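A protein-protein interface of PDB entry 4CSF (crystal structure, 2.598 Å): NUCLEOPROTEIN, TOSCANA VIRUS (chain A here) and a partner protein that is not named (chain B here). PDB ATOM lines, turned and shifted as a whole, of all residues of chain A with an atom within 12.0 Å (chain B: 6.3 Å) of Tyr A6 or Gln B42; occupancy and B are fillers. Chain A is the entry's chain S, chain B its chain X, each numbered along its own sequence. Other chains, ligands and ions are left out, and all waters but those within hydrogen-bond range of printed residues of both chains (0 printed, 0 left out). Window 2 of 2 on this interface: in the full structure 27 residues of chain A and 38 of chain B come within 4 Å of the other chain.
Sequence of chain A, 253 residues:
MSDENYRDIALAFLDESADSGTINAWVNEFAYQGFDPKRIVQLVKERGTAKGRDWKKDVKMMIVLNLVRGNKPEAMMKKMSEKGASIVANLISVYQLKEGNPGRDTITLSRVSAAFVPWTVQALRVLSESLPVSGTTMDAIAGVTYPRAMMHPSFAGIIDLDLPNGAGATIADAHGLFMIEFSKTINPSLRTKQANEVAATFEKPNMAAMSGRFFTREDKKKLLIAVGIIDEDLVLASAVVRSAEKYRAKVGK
The guanidinium group of Arg A7 lies within salt-bridge range of the side-chain carboxylate of Asp A8. NH1 of Arg B39 sits at hydrogen-bond distance from OE1 of Gln B42 (3.0 Å). The side-chain carboxylate (OE2) of Glu B46 is in hydrogen-bond range of the side-chain amide nitrogen (NE2) of Gln B42.
Tyr A6 touches Lys B38. CB of Tyr A6 touches CG2 of Val B41, at 3.5 Å. Tyr A6 touches Phe B214 (O to CZ, 3.6 Å). O of Phe B214 touches CG of Arg A7, at 3.2 Å. CD1 of Phe B215 touches CG of Arg A7 (3.95 Å). CB of Ala A10 touches CE2 of Phe B214, 3.9 Å away. Leu A11 touches Phe B215. CE1 of Phe B116 touches CE1 of Phe A13, at 3.4 Å.
Tyr A6 touches four residues of chain B. Of the printed residues of chain B, Ala A10 touches Phe B214 (3.9 Å). Ala A12 touches none of the printed residues of chain B. Of chain A, only Tyr A6 comes within 4 Å of Lys B38. No residue of chain A comes within 4 Å of Arg B39. No residue of chain A comes within 4 Å of Ile B40. Val B41 touches one residue of chain A. Of chain A, only Tyr A6 (3.1 Å) comes within 4 Å of Gln B42. No residue of chain A comes within 4 Å of Leu B43. No residue of chain A comes within 4 Å of Lys B45. Glu B46 touches none of the printed residues of chain A. Printed residues of chain A within 4 Å of Phe B215: Arg A7 (3.95 Å) and Leu A11 (3.5 Å). The nearest residue of chain B that does not touch Tyr A6 is Glu B46 (4.2 Å). The nearest residue of chain A that does not touch Gln B42 is Ile A9 (6.4 Å). The nearest printed residue of chain A that does not touch Phe B214 is Asp A8 (5.7 Å).
Of the 12 printed residues of chain A, 5 touch a printed residue of chain B. Of the 14 printed residues of chain B, 6 touch a printed residue of chain A. Hydrophobic or aromatic side chains of chain B within 4 Å of the printed part of chain A: Val B41, Phe B116, Phe B214 and Phe B215.
The side-chain amide nitrogen (NE2) of Gln B42 is in hydrogen-bond range of the side-chain hydroxyl (OH) of Tyr A6 (3.1 Å).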
ATOM      1  N   GLU A   4      -1.497   0.332  24.676  1.00  0.00           N
ATOM      2  CA  GLU A   4      -1.779   1.741  24.926  1.00  0.00           C
ATOM      3  C   GLU A   4      -1.616   2.526  23.630  1.00  0.00           C
ATOM      4  O   GLU A   4      -2.276   3.544  23.413  1.00  0.00           O
ATOM      5  CB  GLU A   4      -0.850   2.289  26.006  1.00  0.00           C
ATOM      6  N   ASN A   5      -0.728   2.039  22.771  1.00  0.00           N
ATOM      7  CA  ASN A   5      -0.522   2.650  21.468  1.00  0.00           C
ATOM      8  C   ASN A   5      -1.180   1.862  20.345  1.00  0.00           C
ATOM      9  O   ASN A   5      -1.357   2.389  19.251  1.00  0.00           O
ATOM     10  CB  ASN A   5       0.968   2.884  21.178  1.00  0.00           C
ATOM     11  CG  ASN A   5       1.833   1.675  21.497  1.00  0.00           C
ATOM     12  OD1 ASN A   5       2.457   1.611  22.558  1.00  0.00           O
ATOM     13  ND2 ASN A   5       1.882   0.718  20.576  1.00  0.00           N
ATOM     14  N   TYR A   6      -1.549   0.609  20.603  1.00  0.00           N
ATOM     15  CA  TYR A   6      -2.344  -0.115  19.618  1.00  0.00           C
ATOM     16  C   TYR A   6      -3.715   0.544  19.527  1.00  0.00           C
ATOM     17  O   TYR A   6      -4.330   0.577  18.463  1.00  0.00           O
ATOM     18  CB  TYR A   6      -2.456  -1.601  19.963  1.00  0.00           C
ATOM     19  CG  TYR A   6      -1.125  -2.310  19.895  1.00  0.00           C
ATOM     20  CD1 TYR A   6      -0.268  -2.110  18.822  1.00  0.00           C
ATOM     21  CD2 TYR A   6      -0.718  -3.166  20.904  1.00  0.00           C
ATOM     22  CE1 TYR A   6       0.956  -2.744  18.757  1.00  0.00           C
ATOM     23  CE2 TYR A   6       0.504  -3.807  20.851  1.00  0.00           C
ATOM     24  CZ  TYR A   6       1.339  -3.592  19.775  1.00  0.00           C
ATOM     25  OH  TYR A   6       2.558  -4.227  19.711  1.00  0.00           O
ATOM     26  N   ARG A   7      -4.174   1.090  20.648  1.00  0.00           N
ATOM     27  CA  ARG A   7      -5.448   1.797  20.691  1.00  0.00           C
ATOM     28  C   ARG A   7      -5.372   3.067  19.851  1.00  0.00           C
ATOM     29  O   ARG A   7      -6.287   3.375  19.085  1.00  0.00           O
ATOM     30  CB  ARG A   7      -5.821   2.129  22.135  1.00  0.00           C
ATOM     31  CG  ARG A   7      -7.238   2.627  22.315  1.00  0.00           C
ATOM     32  CD  ARG A   7      -7.269   4.091  22.708  1.00  0.00           C
ATOM     33  NE  ARG A   7      -6.554   4.349  23.955  1.00  0.00           N
ATOM     34  CZ  ARG A   7      -6.483   5.539  24.546  1.00  0.00           C
ATOM     35  NH1 ARG A   7      -7.089   6.586  24.003  1.00  0.00           N
ATOM     36  NH2 ARG A   7      -5.809   5.682  25.682  1.00  0.00           N
ATOM     37  N   ASP A   8      -4.266   3.792  19.987  1.00  0.00           N
ATOM     38  CA  ASP A   8      -4.065   5.035  19.247  1.00  0.00           C
ATOM     39  C   ASP A   8      -3.856   4.794  17.751  1.00  0.00           C
ATOM     40  O   ASP A   8      -4.232   5.627  16.925  1.00  0.00           O
ATOM     41  CB  ASP A   8      -2.893   5.824  19.831  1.00  0.00           C
ATOM     42  CG  ASP A   8      -3.176   6.338  21.233  1.00  0.00           C
ATOM     43  OD1 ASP A   8      -4.327   6.747  21.503  1.00  0.00           O
ATOM     44  OD2 ASP A   8      -2.242   6.339  22.064  1.00  0.00           O
ATOM     45  N   ILE A   9      -3.256   3.655  17.411  1.00  0.00           N
ATOM     46  CA  ILE A   9      -3.090   3.256  16.016  1.00  0.00           C
ATOM     47  C   ILE A   9      -4.450   3.086  15.339  1.00  0.00           C
ATOM     48  O   ILE A   9      -4.688   3.632  14.260  1.00  0.00           O
ATOM     49  CB  ILE A   9      -2.279   1.945  15.887  1.00  0.00           C
ATOM     50  CG1 ILE A   9      -0.806   2.188  16.229  1.00  0.00           C
ATOM     51  CG2 ILE A   9      -2.394   1.372  14.480  1.00  0.00           C
ATOM     52  CD1 ILE A   9       0.035   0.929  16.260  1.00  0.00           C
ATOM     53  N   ALA A  10      -5.335   2.328  15.982  1.00  0.00           N
ATOM     54  CA  ALA A  10      -6.681   2.108  15.468  1.00  0.00           C
ATOM     55  C   ALA A  10      -7.446   3.428  15.379  1.00  0.00           C
ATOM     56  O   ALA A  10      -8.141   3.695  14.392  1.00  0.00           O
ATOM     57  CB  ALA A  10      -7.427   1.117  16.353  1.00  0.00           C
ATOM     58  N   LEU A  11      -7.302   4.247  16.417  1.00  0.00           N
ATOM     59  CA  LEU A  11      -7.993   5.528  16.509  1.00  0.00           C
ATOM     60  C   LEU A  11      -7.549   6.505  15.416  1.00  0.00           C
ATOM     61  O   LEU A  11      -8.319   7.370  14.996  1.00  0.00           O
ATOM     62  CB  LEU A  11      -7.758   6.128  17.899  1.00  0.00           C
ATOM     63  CG  LEU A  11      -8.965   6.432  18.805  1.00  0.00           C
ATOM     64  CD1 LEU A  11     -10.223   5.635  18.464  1.00  0.00           C
ATOM     65  CD2 LEU A  11      -8.611   6.319  20.287  1.00  0.00           C
ATOM     66  N   ALA A  12      -6.311   6.357  14.952  1.00  0.00           N
ATOM     67  CA  ALA A  12      -5.771   7.231  13.912  1.00  0.00           C
ATOM     68  C   ALA A  12      -6.380   6.958  12.533  1.00  0.00           C
ATOM     69  O   ALA A  12      -6.272   7.784  11.626  1.00  0.00           O
ATOM     70  CB  ALA A  12      -4.258   7.111  13.858  1.00  0.00           C
ATOM     71  N   PHE A  13      -7.017   5.800  12.380  1.00  0.00           N
ATOM     72  CA  PHE A  13      -7.664   5.451  11.120  1.00  0.00           C
ATOM     73  C   PHE A  13      -8.905   6.295  10.867  1.00  0.00           C
ATOM     74  O   PHE A  13      -9.461   6.275   9.770  1.00  0.00           O
ATOM     75  CB  PHE A  13      -8.003   3.960  11.074  1.00  0.00           C
ATOM     76  CG  PHE A  13      -6.894   3.114  10.527  1.00  0.00           C
ATOM     77  CD1 PHE A  13      -5.823   2.752  11.329  1.00  0.00           C
ATOM     78  CD2 PHE A  13      -6.914   2.695   9.206  1.00  0.00           C
ATOM     79  CE1 PHE A  13      -4.794   1.975  10.825  1.00  0.00           C
ATOM     80  CE2 PHE A  13      -5.887   1.916   8.693  1.00  0.00           C
ATOM     81  CZ  PHE A  13      -4.826   1.556   9.506  1.00  0.00           C
ATOM     82  N   LEU A  14      -9.335   7.029  11.889  1.00  0.00           N
ATOM     83  CA  LEU A  14     -10.411   7.997  11.750  1.00  0.00           C
ATOM     84  C   LEU A  14      -9.998   9.055  10.737  1.00  0.00           C
ATOM     85  O   LEU A  14     -10.790   9.473   9.891  1.00  0.00           O
ATOM     86  CB  LEU A  14     -10.676   8.677  13.093  1.00  0.00           C
ATOM     87  CG  LEU A  14     -12.107   9.114  13.450  1.00  0.00           C
ATOM     88  CD1 LEU A  14     -12.153  10.404  14.290  1.00  0.00           C
ATOM     89  CD2 LEU A  14     -13.075   9.157  12.256  1.00  0.00           C
ATOM     90  N   GLU A  16      -7.548   8.630   8.607  1.00  0.00           N
ATOM     91  CA  GLU A  16      -6.935   7.978   7.458  1.00  0.00           C
ATOM     92  C   GLU A  16      -7.864   8.097   6.248  1.00  0.00           C
ATOM     93  O   GLU A  16      -9.089   8.120   6.397  1.00  0.00           O
ATOM     94  CB  GLU A  16      -6.618   6.517   7.780  1.00  0.00           C
ATOM     95  CG  GLU A  16      -5.574   5.896   6.871  1.00  0.00           C
ATOM     96  CD  GLU A  16      -4.149   6.199   7.285  1.00  0.00           C
ATOM     97  OE1 GLU A  16      -3.862   6.176   8.499  1.00  0.00           O
ATOM     98  OE2 GLU A  16      -3.307   6.440   6.394  1.00  0.00           O
ATOM     99  N   PRO B  37      -8.907  -6.862  20.180  1.00  0.00           N
ATOM    100  CA  PRO B  37      -8.666  -5.870  19.124  1.00  0.00           C
ATOM    101  C   PRO B  37      -7.225  -5.368  19.158  1.00  0.00           C
ATOM    102  O   PRO B  37      -6.606  -5.193  18.106  1.00  0.00           O
ATOM    103  CB  PRO B  37      -9.626  -4.731  19.486  1.00  0.00           C
ATOM    104  CG  PRO B  37     -10.715  -5.381  20.275  1.00  0.00           C
ATOM    105  CD  PRO B  37     -10.053  -6.499  21.035  1.00  0.00           C
ATOM    106  N   LYS B  38      -6.711  -5.148  20.366  1.00  0.00           N
ATOM    107  CA  LYS B  38      -5.333  -4.710  20.577  1.00  0.00           C
ATOM    108  C   LYS B  38      -4.344  -5.650  19.895  1.00  0.00           C
ATOM    109  O   LYS B  38      -3.428  -5.210  19.199  1.00  0.00           O
ATOM    110  CB  LYS B  38      -5.030  -4.646  22.075  1.00  0.00           C
ATOM    111  CG  LYS B  38      -3.591  -4.311  22.401  1.00  0.00           C
ATOM    112  CD  LYS B  38      -3.115  -5.030  23.657  1.00  0.00           C
ATOM    113  CE  LYS B  38      -3.975  -4.690  24.864  1.00  0.00           C
ATOM    114  NZ  LYS B  38      -3.538  -5.432  26.081  1.00  0.00           N
ATOM    115  N   ARG B  39      -4.548  -6.949  20.099  1.00  0.00           N
ATOM    116  CA  ARG B  39      -3.697  -7.980  19.518  1.00  0.00           C
ATOM    117  C   ARG B  39      -3.824  -7.987  17.992  1.00  0.00           C
ATOM    118  O   ARG B  39      -2.860  -8.267  17.275  1.00  0.00           O
ATOM    119  CB  ARG B  39      -4.073  -9.348  20.101  1.00  0.00           C
ATOM    120  CG  ARG B  39      -3.160 -10.500  19.698  1.00  0.00           C
ATOM    121  CD  ARG B  39      -1.781 -10.399  20.342  1.00  0.00           C
ATOM    122  NE  ARG B  39      -0.948 -11.554  20.013  1.00  0.00           N
ATOM    123  CZ  ARG B  39       0.343 -11.483  19.697  1.00  0.00           C
ATOM    124  NH1 ARG B  39       0.959 -10.306  19.666  1.00  0.00           N
ATOM    125  NH2 ARG B  39       1.022 -12.588  19.410  1.00  0.00           N
ATOM    126  N   ILE B  40      -5.018  -7.660  17.504  1.00  0.00           N
ATOM    127  CA  ILE B  40      -5.282  -7.649  16.069  1.00  0.00           C
ATOM    128  C   ILE B  40      -4.487  -6.564  15.338  1.00  0.00           C
ATOM    129  O   ILE B  40      -3.809  -6.848  14.349  1.00  0.00           O
ATOM    130  CB  ILE B  40      -6.796  -7.510  15.758  1.00  0.00           C
ATOM    131  CG1 ILE B  40      -7.561  -8.744  16.240  1.00  0.00           C
ATOM    132  CG2 ILE B  40      -7.025  -7.298  14.266  1.00  0.00           C
ATOM    133  CD1 ILE B  40      -7.113 -10.041  15.583  1.00  0.00           C
ATOM    134  N   VAL B  41      -4.562  -5.326  15.821  1.00  0.00           N
ATOM    135  CA  VAL B  41      -3.833  -4.243  15.159  1.00  0.00           C
ATOM    136  C   VAL B  41      -2.324  -4.468  15.279  1.00  0.00           C
ATOM    137  O   VAL B  41      -1.560  -4.065  14.402  1.00  0.00           O
ATOM    138  CB  VAL B  41      -4.243  -2.817  15.656  1.00  0.00           C
ATOM    139  CG1 VAL B  41      -5.601  -2.839  16.341  1.00  0.00           C
ATOM    140  CG2 VAL B  41      -3.195  -2.231  16.571  1.00  0.00           C
ATOM    141  N   GLN B  42      -1.909  -5.132  16.355  1.00  0.00           N
ATOM    142  CA  GLN B  42      -0.503  -5.459  16.557  1.00  0.00           C
ATOM    143  C   GLN B  42      -0.009  -6.412  15.476  1.00  0.00           C
ATOM    144  O   GLN B  42       0.991  -6.146  14.806  1.00  0.00           O
ATOM    145  CB  GLN B  42      -0.285  -6.090  17.933  1.00  0.00           C
ATOM    146  CG  GLN B  42       1.135  -6.620  18.145  1.00  0.00           C
ATOM    147  CD  GLN B  42       1.374  -7.154  19.548  1.00  0.00           C
ATOM    148  OE1 GLN B  42       0.432  -7.412  20.302  1.00  0.00           O
ATOM    149  NE2 GLN B  42       2.642  -7.319  19.906  1.00  0.00           N
ATOM    150  N   LEU B  43      -0.722  -7.521  15.315  1.00  0.00           N
ATOM    151  CA  LEU B  43      -0.351  -8.554  14.352  1.00  0.00           C
ATOM    152  C   LEU B  43      -0.420  -8.055  12.909  1.00  0.00           C
ATOM    153  O   LEU B  43       0.404  -8.435  12.075  1.00  0.00           O
ATOM    154  CB  LEU B  43      -1.226  -9.798  14.541  1.00  0.00           C
ATOM    155  CG  LEU B  43      -0.996 -10.555  15.855  1.00  0.00           C
ATOM    156  CD1 LEU B  43      -1.993 -11.688  16.030  1.00  0.00           C
ATOM    157  CD2 LEU B  43       0.432 -11.080  15.916  1.00  0.00           C
ATOM    158  N   VAL B  44      -1.398  -7.199  12.621  1.00  0.00           N
ATOM    159  CA  VAL B  44      -1.525  -6.605  11.295  1.00  0.00           C
ATOM    160  C   VAL B  44      -0.304  -5.744  10.970  1.00  0.00           C
ATOM    161  O   VAL B  44       0.301  -5.886   9.904  1.00  0.00           O
ATOM    162  CB  VAL B  44      -2.801  -5.753  11.176  1.00  0.00           C
ATOM    163  CG1 VAL B  44      -2.725  -4.861   9.950  1.00  0.00           C
ATOM    164  CG2 VAL B  44      -4.034  -6.644  11.122  1.00  0.00           C
ATOM    165  N   LYS B  45       0.056  -4.859  11.898  1.00  0.00           N
ATOM    166  CA  LYS B  45       1.201  -3.975  11.709  1.00  0.00           C
ATOM    167  C   LYS B  45       2.512  -4.753  11.631  1.00  0.00           C
ATOM    168  O   LYS B  45       3.363  -4.460  10.789  1.00  0.00           O
ATOM    169  CB  LYS B  45       1.278  -2.931  12.825  1.00  0.00           C
ATOM    170  CG  LYS B  45       2.413  -1.932  12.640  1.00  0.00           C
ATOM    171  CD  LYS B  45       2.606  -1.066  13.872  1.00  0.00           C
ATOM    172  CE  LYS B  45       3.807  -0.144  13.717  1.00  0.00           C
ATOM    173  NZ  LYS B  45       4.072   0.624  14.967  1.00  0.00           N
ATOM    174  N   GLU B  46       2.670  -5.744  12.508  1.00  0.00           N
ATOM    175  CA  GLU B  46       3.881  -6.561  12.530  1.00  0.00           C
ATOM    176  C   GLU B  46       4.043  -7.377  11.245  1.00  0.00           C
ATOM    177  O   GLU B  46       5.079  -7.301  10.580  1.00  0.00           O
ATOM    178  CB  GLU B  46       3.896  -7.488  13.752  1.00  0.00           C
ATOM    179  CG  GLU B  46       4.172  -6.780  15.077  1.00  0.00           C
ATOM    180  CD  GLU B  46       4.123  -7.725  16.265  1.00  0.00           C
ATOM    181  OE1 GLU B  46       3.904  -8.939  16.053  1.00  0.00           O
ATOM    182  OE2 GLU B  46       4.304  -7.254  17.409  1.00  0.00           O
ATOM    183  N   ARG B  47       3.017  -8.151  10.898  1.00  0.00           N
ATOM    184  CA  ARG B  47       3.077  -9.012   9.720  1.00  0.00           C
ATOM    185  C   ARG B  47       3.151  -8.209   8.425  1.00  0.00           C
ATOM    186  O   ARG B  47       3.789  -8.637   7.463  1.00  0.00           O
ATOM    187  CB  ARG B  47       1.890  -9.977   9.687  1.00  0.00           C
ATOM    188  CG  ARG B  47       1.847 -10.960  10.852  1.00  0.00           C
ATOM    189  CD  ARG B  47       1.130 -12.238  10.458  1.00  0.00           C
ATOM    190  NE  ARG B  47      -0.075 -12.495  11.243  1.00  0.00           N
ATOM    191  CZ  ARG B  47      -0.113 -13.277  12.318  1.00  0.00           C
ATOM    192  NH1 ARG B  47       0.989 -13.875  12.749  1.00  0.00           N
ATOM    193  NH2 ARG B  47      -1.255 -13.461  12.966  1.00  0.00           N
ATOM    194  N   PHE B 116     -10.266  -1.930  13.470  1.00  0.00           N
ATOM    195  CA  PHE B 116     -10.042  -0.662  12.783  1.00  0.00           C
ATOM    196  C   PHE B 116     -11.360   0.006  12.422  1.00  0.00           C
ATOM    197  O   PHE B 116     -11.486   0.632  11.369  1.00  0.00           O
ATOM    198  CB  PHE B 116      -9.188  -0.874  11.531  1.00  0.00           C
ATOM    199  CG  PHE B 116      -7.802  -1.376  11.825  1.00  0.00           C
ATOM    200  CD1 PHE B 116      -6.766  -0.486  12.092  1.00  0.00           C
ATOM    201  CD2 PHE B 116      -7.533  -2.739  11.845  1.00  0.00           C
ATOM    202  CE1 PHE B 116      -5.485  -0.948  12.370  1.00  0.00           C
ATOM    203  CE2 PHE B 116      -6.254  -3.208  12.122  1.00  0.00           C
ATOM    204  CZ  PHE B 116      -5.231  -2.310  12.382  1.00  0.00           C
ATOM    205  N   PHE B 214     -11.489  -1.639  24.774  1.00  0.00           N
ATOM    206  CA  PHE B 214     -10.373  -1.264  23.914  1.00  0.00           C
ATOM    207  C   PHE B 214     -10.392   0.248  23.719  1.00  0.00           C
ATOM    208  O   PHE B 214      -9.374   0.922  23.883  1.00  0.00           O
ATOM    209  CB  PHE B 214     -10.471  -1.994  22.569  1.00  0.00           C
ATOM    210  CG  PHE B 214      -9.354  -1.667  21.602  1.00  0.00           C
ATOM    211  CD1 PHE B 214      -8.021  -1.834  21.965  1.00  0.00           C
ATOM    212  CD2 PHE B 214      -9.640  -1.218  20.317  1.00  0.00           C
ATOM    213  CE1 PHE B 214      -6.992  -1.539  21.069  1.00  0.00           C
ATOM    214  CE2 PHE B 214      -8.619  -0.924  19.414  1.00  0.00           C
ATOM    215  CZ  PHE B 214      -7.293  -1.086  19.793  1.00  0.00           C
ATOM    216  N   PHE B 215     -11.565   0.775  23.383  1.00  0.00           N
ATOM    217  CA  PHE B 215     -11.762   2.217  23.295  1.00  0.00           C
ATOM    218  C   PHE B 215     -12.367   2.744  24.590  1.00  0.00           C
ATOM    219  O   PHE B 215     -13.224   2.095  25.189  1.00  0.00           O
ATOM    220  CB  PHE B 215     -12.672   2.560  22.115  1.00  0.00           C
ATOM    221  CG  PHE B 215     -12.072   2.234  20.778  1.00  0.00           C
ATOM    222  CD1 PHE B 215     -10.750   2.547  20.504  1.00  0.00           C
ATOM    223  CD2 PHE B 215     -12.821   1.604  19.800  1.00  0.00           C
ATOM    224  CE1 PHE B 215     -10.187   2.245  19.272  1.00  0.00           C
ATOM    225  CE2 PHE B 215     -12.264   1.300  18.567  1.00  0.00           C
ATOM    226  CZ  PHE B 215     -10.947   1.621  18.305  1.00  0.00           C
